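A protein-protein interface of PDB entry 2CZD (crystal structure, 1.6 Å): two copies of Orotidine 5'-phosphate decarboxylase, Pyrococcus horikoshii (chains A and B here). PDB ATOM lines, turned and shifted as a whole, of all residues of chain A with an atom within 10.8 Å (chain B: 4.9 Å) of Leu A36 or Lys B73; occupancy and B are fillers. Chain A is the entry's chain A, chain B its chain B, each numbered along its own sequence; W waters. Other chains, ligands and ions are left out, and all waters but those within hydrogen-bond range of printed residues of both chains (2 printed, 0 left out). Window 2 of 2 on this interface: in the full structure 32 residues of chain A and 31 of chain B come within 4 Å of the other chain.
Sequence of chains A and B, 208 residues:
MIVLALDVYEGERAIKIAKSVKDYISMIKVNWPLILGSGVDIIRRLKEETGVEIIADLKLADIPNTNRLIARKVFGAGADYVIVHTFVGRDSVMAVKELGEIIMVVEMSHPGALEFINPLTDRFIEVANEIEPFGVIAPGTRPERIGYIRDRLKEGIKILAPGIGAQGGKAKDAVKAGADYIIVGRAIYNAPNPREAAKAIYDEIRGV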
ATOM      1  N   LEU A   6      25.074  10.680 -23.463  1.00  0.00           N
ATOM      2  CA  LEU A   6      26.313   9.890 -23.465  1.00  0.00           C
ATOM      3  C   LEU A   6      26.081   8.489 -24.036  1.00  0.00           C
ATOM      4  O   LEU A   6      26.111   7.473 -23.321  1.00  0.00           O
ATOM      5  CB  LEU A   6      26.851   9.842 -22.023  1.00  0.00           C
ATOM      6  CG  LEU A   6      28.243   9.217 -21.856  1.00  0.00           C
ATOM      7  CD1 LEU A   6      29.278   9.916 -22.721  1.00  0.00           C
ATOM      8  CD2 LEU A   6      28.651   9.308 -20.402  1.00  0.00           C
ATOM      9  N   VAL A   8      27.592   6.186 -25.567  1.00  0.00           N
ATOM     10  CA  VAL A   8      28.870   5.482 -25.722  1.00  0.00           C
ATOM     11  C   VAL A   8      28.641   4.275 -24.824  1.00  0.00           C
ATOM     12  O   VAL A   8      28.522   4.403 -23.610  1.00  0.00           O
ATOM     13  CB  VAL A   8      29.995   6.377 -25.200  1.00  0.00           C
ATOM     14  CG1 VAL A   8      31.291   5.608 -25.124  1.00  0.00           C
ATOM     15  CG2 VAL A   8      30.135   7.603 -26.120  1.00  0.00           C
ATOM     16  N   TYR A   9      28.612   3.095 -25.423  1.00  0.00           N
ATOM     17  CA  TYR A   9      28.218   1.919 -24.673  1.00  0.00           C
ATOM     18  C   TYR A   9      29.254   1.078 -23.966  1.00  0.00           C
ATOM     19  O   TYR A   9      28.917   0.076 -23.319  1.00  0.00           O
ATOM     20  CB  TYR A   9      27.302   1.093 -25.571  1.00  0.00           C
ATOM     21  CG  TYR A   9      26.168   1.943 -26.077  1.00  0.00           C
ATOM     22  CD1 TYR A   9      25.904   2.066 -27.450  1.00  0.00           C
ATOM     23  CD2 TYR A   9      25.407   2.702 -25.185  1.00  0.00           C
ATOM     24  CE1 TYR A   9      24.905   2.938 -27.913  1.00  0.00           C
ATOM     25  CE2 TYR A   9      24.422   3.564 -25.626  1.00  0.00           C
ATOM     26  CZ  TYR A   9      24.167   3.682 -26.978  1.00  0.00           C
ATOM     27  OH  TYR A   9      23.151   4.514 -27.393  1.00  0.00           O
ATOM     28  N   GLU A  10      30.509   1.502 -24.070  1.00  0.00           N
ATOM     29  CA  GLU A  10      31.598   0.861 -23.348  1.00  0.00           C
ATOM     30  C   GLU A  10      31.724   1.813 -22.149  1.00  0.00           C
ATOM     31  O   GLU A  10      32.124   2.969 -22.299  1.00  0.00           O
ATOM     32  CB  GLU A  10      32.863   0.840 -24.201  1.00  0.00           C
ATOM     33  CG  GLU A  10      32.684   0.154 -25.555  1.00  0.00           C
ATOM     34  CD  GLU A  10      32.045   1.026 -26.627  1.00  0.00           C
ATOM     35  OE1 GLU A  10      31.366   0.458 -27.511  1.00  0.00           O
ATOM     36  OE2 GLU A  10      32.232   2.261 -26.605  1.00  0.00           O
ATOM     37  N   GLY A  11      31.351   1.326 -20.968  1.00  0.00           N
ATOM     38  CA  GLY A  11      31.314   2.165 -19.786  1.00  0.00           C
ATOM     39  C   GLY A  11      32.523   2.983 -19.423  1.00  0.00           C
ATOM     40  O   GLY A  11      32.391   4.133 -19.003  1.00  0.00           O
ATOM     41  N   VAL A  30      21.964   9.018 -19.636  1.00  0.00           N
ATOM     42  CA  VAL A  30      22.340   7.650 -19.997  1.00  0.00           C
ATOM     43  C   VAL A  30      21.106   6.853 -20.402  1.00  0.00           C
ATOM     44  O   VAL A  30      20.004   7.115 -19.918  1.00  0.00           O
ATOM     45  CB  VAL A  30      23.029   6.936 -18.826  1.00  0.00           C
ATOM     46  CG1 VAL A  30      24.275   7.727 -18.400  1.00  0.00           C
ATOM     47  CG2 VAL A  30      22.071   6.762 -17.682  1.00  0.00           C
ATOM     48  N   ASN A  31      21.275   5.877 -21.278  1.00  0.00           N
ATOM     49  CA  ASN A  31      20.107   5.109 -21.714  1.00  0.00           C
ATOM     50  C   ASN A  31      20.228   3.627 -21.397  1.00  0.00           C
ATOM     51  O   ASN A  31      21.225   3.193 -20.802  1.00  0.00           O
ATOM     52  CB  ASN A  31      19.864   5.332 -23.207  1.00  0.00           C
ATOM     53  CG  ASN A  31      21.011   4.854 -24.064  1.00  0.00           C
ATOM     54  OD1 ASN A  31      21.895   4.128 -23.588  1.00  0.00           O
ATOM     55  ND2 ASN A  31      21.003   5.241 -25.343  1.00  0.00           N
ATOM     56  N   TRP A  32      19.231   2.841 -21.801  1.00  0.00           N
ATOM     57  CA  TRP A  32      19.275   1.415 -21.496  1.00  0.00           C
ATOM     58  C   TRP A  32      20.510   0.682 -22.034  1.00  0.00           C
ATOM     59  O   TRP A  32      21.101  -0.115 -21.318  1.00  0.00           O
ATOM     60  CB  TRP A  32      17.995   0.721 -21.974  1.00  0.00           C
ATOM     61  CG  TRP A  32      16.799   0.881 -21.041  1.00  0.00           C
ATOM     62  CD1 TRP A  32      15.584   1.446 -21.355  1.00  0.00           C
ATOM     63  CD2 TRP A  32      16.673   0.395 -19.700  1.00  0.00           C
ATOM     64  NE1 TRP A  32      14.716   1.335 -20.292  1.00  0.00           N
ATOM     65  CE2 TRP A  32      15.353   0.701 -19.262  1.00  0.00           C
ATOM     66  CE3 TRP A  32      17.534  -0.263 -18.821  1.00  0.00           C
ATOM     67  CZ2 TRP A  32      14.890   0.368 -17.988  1.00  0.00           C
ATOM     68  CZ3 TRP A  32      17.064  -0.597 -17.538  1.00  0.00           C
ATOM     69  CH2 TRP A  32      15.756  -0.278 -17.146  1.00  0.00           C
ATOM     70  N   PRO A  33      20.905   0.927 -23.288  1.00  0.00           N
ATOM     71  CA  PRO A  33      22.096   0.228 -23.798  1.00  0.00           C
ATOM     72  C   PRO A  33      23.326   0.416 -22.900  1.00  0.00           C
ATOM     73  O   PRO A  33      24.070  -0.537 -22.652  1.00  0.00           O
ATOM     74  CB  PRO A  33      22.280   0.837 -25.183  1.00  0.00           C
ATOM     75  CG  PRO A  33      20.810   1.004 -25.657  1.00  0.00           C
ATOM     76  CD  PRO A  33      20.166   1.593 -24.382  1.00  0.00           C
ATOM     77  N   LEU A  34      23.562   1.629 -22.413  1.00  0.00           N
ATOM     78  CA  LEU A  34      24.727   1.833 -21.544  1.00  0.00           C
ATOM     79  C   LEU A  34      24.532   1.073 -20.229  1.00  0.00           C
ATOM     80  O   LEU A  34      25.449   0.398 -19.737  1.00  0.00           O
ATOM     81  CB  LEU A  34      24.960   3.327 -21.279  1.00  0.00           C
ATOM     82  CG  LEU A  34      26.092   3.663 -20.300  1.00  0.00           C
ATOM     83  CD1 LEU A  34      27.394   2.944 -20.683  1.00  0.00           C
ATOM     84  CD2 LEU A  34      26.317   5.176 -20.307  1.00  0.00           C
ATOM     85  N   ILE A  35      23.339   1.166 -19.666  1.00  0.00           N
ATOM     86  CA  ILE A  35      23.054   0.442 -18.429  1.00  0.00           C
ATOM     87  C   ILE A  35      23.203  -1.080 -18.627  1.00  0.00           C
ATOM     88  O   ILE A  35      23.735  -1.786 -17.745  1.00  0.00           O
ATOM     89  CB  ILE A  35      21.633   0.797 -17.924  1.00  0.00           C
ATOM     90  CG1 ILE A  35      21.645   2.240 -17.393  1.00  0.00           C
ATOM     91  CG2 ILE A  35      21.204  -0.159 -16.803  1.00  0.00           C
ATOM     92  CD1 ILE A  35      20.239   2.834 -17.175  1.00  0.00           C
ATOM     93  N   LEU A  36      22.781  -1.591 -19.784  1.00  0.00           N
ATOM     94  CA  LEU A  36      22.896  -3.027 -20.036  1.00  0.00           C
ATOM     95  C   LEU A  36      24.343  -3.455 -20.237  1.00  0.00           C
ATOM     96  O   LEU A  36      24.731  -4.549 -19.824  1.00  0.00           O
ATOM     97  CB  LEU A  36      22.088  -3.425 -21.265  1.00  0.00           C
ATOM     98  CG  LEU A  36      20.576  -3.253 -21.120  1.00  0.00           C
ATOM     99  CD1 LEU A  36      19.915  -3.503 -22.457  1.00  0.00           C
ATOM    100  CD2 LEU A  36      20.047  -4.235 -20.070  1.00  0.00           C
ATOM    101  N   GLY A  37      25.144  -2.581 -20.843  1.00  0.00           N
ATOM    102  CA  GLY A  37      26.531  -2.937 -21.083  1.00  0.00           C
ATOM    103  C   GLY A  37      27.455  -2.863 -19.881  1.00  0.00           C
ATOM    104  O   GLY A  37      28.332  -3.713 -19.709  1.00  0.00           O
ATOM    105  N   SER A  38      27.281  -1.851 -19.041  1.00  0.00           N
ATOM    106  CA  SER A  38      28.153  -1.684 -17.892  1.00  0.00           C
ATOM    107  C   SER A  38      27.520  -1.972 -16.549  1.00  0.00           C
ATOM    108  O   SER A  38      28.220  -2.017 -15.535  1.00  0.00           O
ATOM    109  CB  SER A  38      28.679  -0.253 -17.857  1.00  0.00           C
ATOM    110  OG  SER A  38      29.344   0.049 -19.057  1.00  0.00           O
ATOM    111  N   GLY A  39      26.204  -2.186 -16.544  1.00  0.00           N
ATOM    112  CA  GLY A  39      25.498  -2.380 -15.293  1.00  0.00           C
ATOM    113  C   GLY A  39      24.995  -1.034 -14.783  1.00  0.00           C
ATOM    114  O   GLY A  39      25.601   0.016 -15.045  1.00  0.00           O
ATOM    115  N   VAL A  40      23.914  -1.062 -14.007  1.00  0.00           N
ATOM    116  CA  VAL A  40      23.306   0.163 -13.494  1.00  0.00           C
ATOM    117  C   VAL A  40      24.258   0.966 -12.597  1.00  0.00           C
ATOM    118  O   VAL A  40      24.083   2.177 -12.427  1.00  0.00           O
ATOM    119  CB  VAL A  40      21.991  -0.173 -12.749  1.00  0.00           C
ATOM    120  CG1 VAL A  40      22.309  -0.812 -11.391  1.00  0.00           C
ATOM    121  CG2 VAL A  40      21.115   1.073 -12.613  1.00  0.00           C
ATOM    122  N   ASP A  41      25.293   0.310 -12.062  1.00  0.00           N
ATOM    123  CA  ASP A  41      26.254   1.020 -11.214  1.00  0.00           C
ATOM    124  C   ASP A  41      27.026   2.096 -12.000  1.00  0.00           C
ATOM    125  O   ASP A  41      27.660   2.977 -11.407  1.00  0.00           O
ATOM    126  CB  ASP A  41      27.245   0.030 -10.586  1.00  0.00           C
ATOM    127  CG  ASP A  41      28.113   0.675  -9.516  1.00  0.00           C
ATOM    128  OD1 ASP A  41      29.356   0.590  -9.642  1.00  0.00           O
ATOM    129  OD2 ASP A  41      27.554   1.263  -8.556  1.00  0.00           O
ATOM    130  N   ILE A  42      26.967   2.032 -13.329  1.00  0.00           N
ATOM    131  CA  ILE A  42      27.645   3.040 -14.136  1.00  0.00           C
ATOM    132  C   ILE A  42      27.120   4.428 -13.793  1.00  0.00           C
ATOM    133  O   ILE A  42      27.835   5.420 -13.938  1.00  0.00           O
ATOM    134  CB  ILE A  42      27.477   2.754 -15.662  1.00  0.00           C
ATOM    135  CG1 ILE A  42      28.353   3.698 -16.483  1.00  0.00           C
ATOM    136  CG2 ILE A  42      26.042   2.951 -16.094  1.00  0.00           C
ATOM    137  CD1 ILE A  42      29.816   3.571 -16.174  1.00  0.00           C
ATOM    138  N   ILE A  43      25.873   4.506 -13.313  1.00  0.00           N
ATOM    139  CA  ILE A  43      25.296   5.803 -12.957  1.00  0.00           C
ATOM    140  C   ILE A  43      26.044   6.415 -11.766  1.00  0.00           C
ATOM    141  O   ILE A  43      26.416   7.597 -11.783  1.00  0.00           O
ATOM    142  CB  ILE A  43      23.780   5.630 -12.638  1.00  0.00           C
ATOM    143  CG1 ILE A  43      23.030   5.365 -13.951  1.00  0.00           C
ATOM    144  CG2 ILE A  43      23.226   6.850 -11.889  1.00  0.00           C
ATOM    145  CD1 ILE A  43      21.556   4.951 -13.784  1.00  0.00           C
ATOM    146  N   LEU A  46      29.562   7.516 -12.900  1.00  0.00           N
ATOM    147  CA  LEU A  46      29.593   8.739 -13.687  1.00  0.00           C
ATOM    148  C   LEU A  46      29.462   9.950 -12.770  1.00  0.00           C
ATOM    149  O   LEU A  46      30.176  10.944 -12.938  1.00  0.00           O
ATOM    150  CB  LEU A  46      28.470   8.753 -14.738  1.00  0.00           C
ATOM    151  CG  LEU A  46      28.768   7.824 -15.927  1.00  0.00           C
ATOM    152  CD1 LEU A  46      27.466   7.590 -16.715  1.00  0.00           C
ATOM    153  CD2 LEU A  46      29.857   8.423 -16.848  1.00  0.00           C
ATOM    154  N   ALA A  56      18.453   9.361 -16.235  1.00  0.00           N
ATOM    155  CA  ALA A  56      18.308   8.013 -16.776  1.00  0.00           C
ATOM    156  C   ALA A  56      17.180   8.076 -17.836  1.00  0.00           C
ATOM    157  O   ALA A  56      15.999   8.186 -17.481  1.00  0.00           O
ATOM    158  CB  ALA A  56      17.920   7.033 -15.644  1.00  0.00           C
ATOM    159  N   ASP A  57      17.548   8.025 -19.118  1.00  0.00           N
ATOM    160  CA  ASP A  57      16.580   8.105 -20.231  1.00  0.00           C
ATOM    161  C   ASP A  57      16.041   6.706 -20.480  1.00  0.00           C
ATOM    162  O   ASP A  57      16.466   5.994 -21.411  1.00  0.00           O
ATOM    163  CB  ASP A  57      17.291   8.649 -21.479  1.00  0.00           C
ATOM    164  CG  ASP A  57      16.327   8.980 -22.602  1.00  0.00           C
ATOM    165  OD1 ASP A  57      15.148   8.586 -22.495  1.00  0.00           O
ATOM    166  OD2 ASP A  57      16.748   9.622 -23.598  1.00  0.00           O
ATOM    167  N   LEU A  58      15.087   6.325 -19.647  1.00  0.00           N
ATOM    168  CA  LEU A  58      14.527   4.987 -19.729  1.00  0.00           C
ATOM    169  C   LEU A  58      13.198   4.944 -20.452  1.00  0.00           C
ATOM    170  O   LEU A  58      12.806   3.886 -20.950  1.00  0.00           O
ATOM    171  CB  LEU A  58      14.324   4.433 -18.312  1.00  0.00           C
ATOM    172  CG  LEU A  58      15.493   4.519 -17.321  1.00  0.00           C
ATOM    173  CD1 LEU A  58      15.070   3.880 -16.002  1.00  0.00           C
ATOM    174  CD2 LEU A  58      16.725   3.801 -17.875  1.00  0.00           C
ATOM    175  N   ILE A  70      11.622  -0.330 -11.011  1.00  0.00           N
ATOM    176  CA  ILE A  70      12.726   0.135 -11.819  1.00  0.00           C
ATOM    177  C   ILE A  70      13.236   1.471 -11.269  1.00  0.00           C
ATOM    178  O   ILE A  70      14.449   1.664 -11.107  1.00  0.00           O
ATOM    179  CB  ILE A  70      12.281   0.325 -13.285  1.00  0.00           C
ATOM    180  CG1 ILE A  70      11.869  -1.021 -13.893  1.00  0.00           C
ATOM    181  CG2 ILE A  70      13.400   0.991 -14.088  1.00  0.00           C
ATOM    182  CD1 ILE A  70      11.084  -0.825 -15.217  1.00  0.00           C
ATOM    183  N   VAL A  74      17.019   2.465 -10.015  1.00  0.00           N
ATOM    184  CA  VAL A  74      17.748   3.465 -10.776  1.00  0.00           C
ATOM    185  C   VAL A  74      18.057   4.735  -9.977  1.00  0.00           C
ATOM    186  O   VAL A  74      19.192   5.241 -10.012  1.00  0.00           O
ATOM    187  CB  VAL A  74      17.000   3.755 -12.080  1.00  0.00           C
ATOM    188  CG1 VAL A  74      17.649   4.957 -12.796  1.00  0.00           C
ATOM    189  CG2 VAL A  74      17.053   2.497 -12.972  1.00  0.00           C
ATOM    190  N   TRP B  32      12.556  -5.804 -16.393  1.00  0.00           N
ATOM    191  CA  TRP B  32      13.703  -4.930 -16.155  1.00  0.00           C
ATOM    192  C   TRP B  32      14.279  -5.061 -14.727  1.00  0.00           C
ATOM    193  O   TRP B  32      15.495  -5.087 -14.552  1.00  0.00           O
ATOM    194  CB  TRP B  32      13.343  -3.455 -16.452  1.00  0.00           C
ATOM    195  CG  TRP B  32      13.337  -3.061 -17.931  1.00  0.00           C
ATOM    196  CD1 TRP B  32      12.311  -2.453 -18.600  1.00  0.00           C
ATOM    197  CD2 TRP B  32      14.434  -3.119 -18.855  1.00  0.00           C
ATOM    198  NE1 TRP B  32      12.701  -2.122 -19.876  1.00  0.00           N
ATOM    199  CE2 TRP B  32      13.998  -2.513 -20.063  1.00  0.00           C
ATOM    200  CE3 TRP B  32      15.739  -3.612 -18.783  1.00  0.00           C
ATOM    201  CZ2 TRP B  32      14.821  -2.388 -21.182  1.00  0.00           C
ATOM    202  CZ3 TRP B  32      16.573  -3.486 -19.911  1.00  0.00           C
ATOM    203  CH2 TRP B  32      16.099  -2.873 -21.094  1.00  0.00           C
ATOM    204  N   ILE B  35      16.718  -7.894 -14.663  1.00  0.00           N
ATOM    205  CA  ILE B  35      17.896  -7.575 -15.471  1.00  0.00           C
ATOM    206  C   ILE B  35      18.787  -6.539 -14.753  1.00  0.00           C
ATOM    207  O   ILE B  35      20.025  -6.618 -14.784  1.00  0.00           O
ATOM    208  CB  ILE B  35      17.452  -7.049 -16.856  1.00  0.00           C
ATOM    209  CG1 ILE B  35      16.812  -8.191 -17.644  1.00  0.00           C
ATOM    210  CG2 ILE B  35      18.644  -6.444 -17.618  1.00  0.00           C
ATOM    211  CD1 ILE B  35      16.137  -7.744 -18.928  1.00  0.00           C
ATOM    212  N   VAL B  40      22.090  -8.384 -17.498  1.00  0.00           N
ATOM    213  CA  VAL B  40      21.394  -8.995 -18.622  1.00  0.00           C
ATOM    214  C   VAL B  40      21.817 -10.466 -18.798  1.00  0.00           C
ATOM    215  O   VAL B  40      21.069 -11.275 -19.357  1.00  0.00           O
ATOM    216  CB  VAL B  40      21.640  -8.188 -19.935  1.00  0.00           C
ATOM    217  CG1 VAL B  40      23.099  -8.297 -20.360  1.00  0.00           C
ATOM    218  CG2 VAL B  40      20.702  -8.673 -21.036  1.00  0.00           C
ATOM    219  N   LEU B  69      19.102  -1.269 -30.520  1.00  0.00           N
ATOM    220  CA  LEU B  69      20.258  -1.548 -29.673  1.00  0.00           C
ATOM    221  C   LEU B  69      19.884  -2.398 -28.458  1.00  0.00           C
ATOM    222  O   LEU B  69      20.611  -3.324 -28.079  1.00  0.00           O
ATOM    223  CB  LEU B  69      20.888  -0.238 -29.209  1.00  0.00           C
ATOM    224  CG  LEU B  69      21.566   0.600 -30.278  1.00  0.00           C
ATOM    225  CD1 LEU B  69      21.924   1.933 -29.692  1.00  0.00           C
ATOM    226  CD2 LEU B  69      22.825  -0.120 -30.783  1.00  0.00           C
ATOM    227  N   ILE B  70      18.754  -2.077 -27.833  1.00  0.00           N
ATOM    228  CA  ILE B  70      18.329  -2.847 -26.679  1.00  0.00           C
ATOM    229  C   ILE B  70      18.004  -4.288 -27.104  1.00  0.00           C
ATOM    230  O   ILE B  70      18.400  -5.251 -26.435  1.00  0.00           O
ATOM    231  CB  ILE B  70      17.089  -2.213 -26.024  1.00  0.00           C
ATOM    232  CG1 ILE B  70      17.457  -0.835 -25.454  1.00  0.00           C
ATOM    233  CG2 ILE B  70      16.538  -3.135 -24.946  1.00  0.00           C
ATOM    234  CD1 ILE B  70      16.223  -0.045 -25.011  1.00  0.00           C
ATOM    235  N   ALA B  71      17.279  -4.431 -28.210  1.00  0.00           N
ATOM    236  CA  ALA B  71      16.893  -5.753 -28.720  1.00  0.00           C
ATOM    237  C   ALA B  71      18.127  -6.598 -29.067  1.00  0.00           C
ATOM    238  O   ALA B  71      18.192  -7.791 -28.758  1.00  0.00           O
ATOM    239  CB  ALA B  71      16.014  -5.588 -29.962  1.00  0.00           C
ATOM    240  N   ARG B  72      19.097  -5.968 -29.715  1.00  0.00           N
ATOM    241  CA  ARG B  72      20.316  -6.667 -30.089  1.00  0.00           C
ATOM    242  C   ARG B  72      20.984  -7.268 -28.861  1.00  0.00           C
ATOM    243  O   ARG B  72      21.382  -8.429 -28.890  1.00  0.00           O
ATOM    244  CB  ARG B  72      21.272  -5.700 -30.797  1.00  0.00           C
ATOM    245  CG  ARG B  72      22.556  -6.322 -31.313  1.00  0.00           C
ATOM    246  CD  ARG B  72      23.185  -5.383 -32.341  1.00  0.00           C
ATOM    247  NE  ARG B  72      24.641  -5.387 -32.284  1.00  0.00           N
ATOM    248  CZ  ARG B  72      25.411  -6.385 -32.701  1.00  0.00           C
ATOM    249  NH1 ARG B  72      24.865  -7.482 -33.221  1.00  0.00           N
ATOM    250  NH2 ARG B  72      26.734  -6.288 -32.598  1.00  0.00           N
ATOM    251  N   LYS B  73      21.106  -6.486 -27.788  1.00  0.00           N
ATOM    252  CA  LYS B  73      21.728  -6.969 -26.552  1.00  0.00           C
ATOM    253  C   LYS B  73      20.910  -8.072 -25.857  1.00  0.00           C
ATOM    254  O   LYS B  73      21.456  -9.084 -25.406  1.00  0.00           O
ATOM    255  CB  LYS B  73      21.894  -5.796 -25.582  1.00  0.00           C
ATOM    256  CG  LYS B  73      22.642  -6.107 -24.308  1.00  0.00           C
ATOM    257  CD  LYS B  73      24.141  -6.222 -24.592  1.00  0.00           C
ATOM    258  CE  LYS B  73      24.938  -6.357 -23.293  1.00  0.00           C
ATOM    259  NZ  LYS B  73      26.394  -6.512 -23.623  1.00  0.00           N
ATOM    260  N   VAL B  74      19.597  -7.872 -25.768  1.00  0.00           N
ATOM    261  CA  VAL B  74      18.720  -8.819 -25.086  1.00  0.00           C
ATOM    262  C   VAL B  74      18.497 -10.120 -25.869  1.00  0.00           C
ATOM    263  O   VAL B  74      18.562 -11.203 -25.281  1.00  0.00           O
ATOM    264  CB  VAL B  74      17.389  -8.098 -24.739  1.00  0.00           C
ATOM    265  CG1 VAL B  74      16.401  -9.045 -24.110  1.00  0.00           C
ATOM    266  CG2 VAL B  74      17.688  -6.970 -23.759  1.00  0.00           C
ATOM    267  N   PHE B  75      18.246 -10.046 -27.175  1.00  0.00           N
ATOM    268  CA  PHE B  75      18.116 -11.286 -27.961  1.00  0.00           C
ATOM    269  C   PHE B  75      19.495 -11.940 -27.932  1.00  0.00           C
ATOM    270  O   PHE B  75      19.619 -13.169 -27.877  1.00  0.00           O
ATOM    271  CB  PHE B  75      17.736 -10.996 -29.414  1.00  0.00           C
ATOM    272  CG  PHE B  75      16.272 -10.658 -29.612  1.00  0.00           C
ATOM    273  CD1 PHE B  75      15.267 -11.532 -29.183  1.00  0.00           C
ATOM    274  CD2 PHE B  75      15.903  -9.505 -30.288  1.00  0.00           C
ATOM    275  CE1 PHE B  75      13.909 -11.248 -29.440  1.00  0.00           C
ATOM    276  CE2 PHE B  75      14.566  -9.216 -30.542  1.00  0.00           C
ATOM    277  CZ  PHE B  75      13.565 -10.087 -30.119  1.00  0.00           C
ATOM    278  N   GLY B  76      20.527 -11.099 -27.957  1.00  0.00           N
ATOM    279  CA  GLY B  76      21.903 -11.575 -27.914  1.00  0.00           C
ATOM    280  C   GLY B  76      22.238 -12.392 -26.675  1.00  0.00           C
ATOM    281  O   GLY B  76      23.019 -13.351 -26.728  1.00  0.00           O
ATOM    282  N   ALA B  77      21.626 -12.025 -25.556  1.00  0.00           N
ATOM    283  CA  ALA B  77      21.843 -12.712 -24.287  1.00  0.00           C
ATOM    284  C   ALA B  77      21.031 -13.995 -24.177  1.00  0.00           C
ATOM    285  O   ALA B  77      21.228 -14.774 -23.247  1.00  0.00           O
ATOM    286  CB  ALA B  77      21.508 -11.769 -23.123  1.00  0.00           C
HETATM  287  O   HOH W   1      21.720  -4.262 -16.316  1.00  0.00           O
HETATM  288  O   HOH W   2      23.553  -5.833 -17.579  1.00  0.00           O
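Hydrophobic or aromatic side chains of chain B that line the printed part of chain A: Trp B32, Ile B35, Leu B69 and Ile B70.
Of the 25 printed residues of chain A, 5 touch a printed residue of chain B.
Printed residues of chain A that touch a printed residue of chain B: Tyr A9, Trp A32, Pro A33, Leu A36 and Ile A70.
Hydrophobic or aromatic side chains of chain A within 4 Å of the printed part of chain B: Tyr A9, Trp A32, Pro A33, Leu A36 and Ile A70.
Along chain A the printed residues that touch a printed residue of chain B span positions 9 to 70.
Among the printed residues, 9 pairs touch across the chains.
Among the printed residues, no Asp or Glu carboxylate lies within 4 Å of a Lys or Arg side-chain nitrogen of the other chain.
Printed residues of chain B within 4 Å of Trp A32: Trp B32 and Ile B70.
Of the printed residues of chain B, Leu A36 touches Trp B32 (3.6 Å), Ile B35 (3.6 Å) and Lys B73 (3.9 Å).
Of the printed residues of chain A, Trp B32 touches Trp A32 (3.5 Å), Leu A36 (3.6 Å) and Ile A70 (3.7 Å).
Ile B70 touches just these residues of chain A: Trp A32 (3.6 Å) and Pro A33 (3.8 Å).
No residue of chain A comes within 4 Å of Ala B71.
Of the printed residues of chain A, Lys B73 touches Leu A36.
No residue of chain A comes within 4 Å of Val B74.
No residue of chain A comes within 4 Å of Gly B76.
The nearest residue of chain A that does not touch Lys B73 is Gly A37 (4.4 Å).
CE1 of Tyr A9 touches CD1 of Leu B69 (3.6 Å).
CZ3 of Trp A32 touches CE3 of Trp B32 (3.5 Å).
Ile B70 touches Trp A32 (CD1 to CB, 3.6 Å).
Pro A33 touches Leu B69.
Ile B70 touches Pro A33 (CG1 to CD, 3.8 Å).
CD2 of Leu A36 touches CZ3 of Trp B32, 3.6 Å away.
Leu A36 touches Ile B35.
Leu A36 touches Lys B73 (O to CE, 3.9 Å).
CD1 of Ile A70 touches CB of Trp B32 (3.7 Å).
The indole nitrogen (NE1) of Trp A32 lies within hydrogen-bond range of the backbone carbonyl oxygen (O) of Leu A58, 3.3 Å away.
The side-chain hydroxyl (OH) of Tyr A9 lies within hydrogen-bond range of the side-chain amide nitrogen (ND2) of Asn A31 (3.1 Å).
Trp B32 touches its own counterpart, Trp A32.
Trp A32 touches Ile B70, and with the chains exchanged Ile A70 touches Trp B32.
Of the 9 pairs that touch across the chains among the printed residues, 3 have their exchanged pair printed and touching as well.
Water W2 lies within hydrogen-bond range of the backbone carbonyl oxygen (O) of Leu A36 (2.8 Å) and the backbone NH (N) of Val B40 (2.9 Å).
Water W1 lies within hydrogen-bond range of O of Ile B35 (3.3 Å) and O of Ile A35 (3.5 Å).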
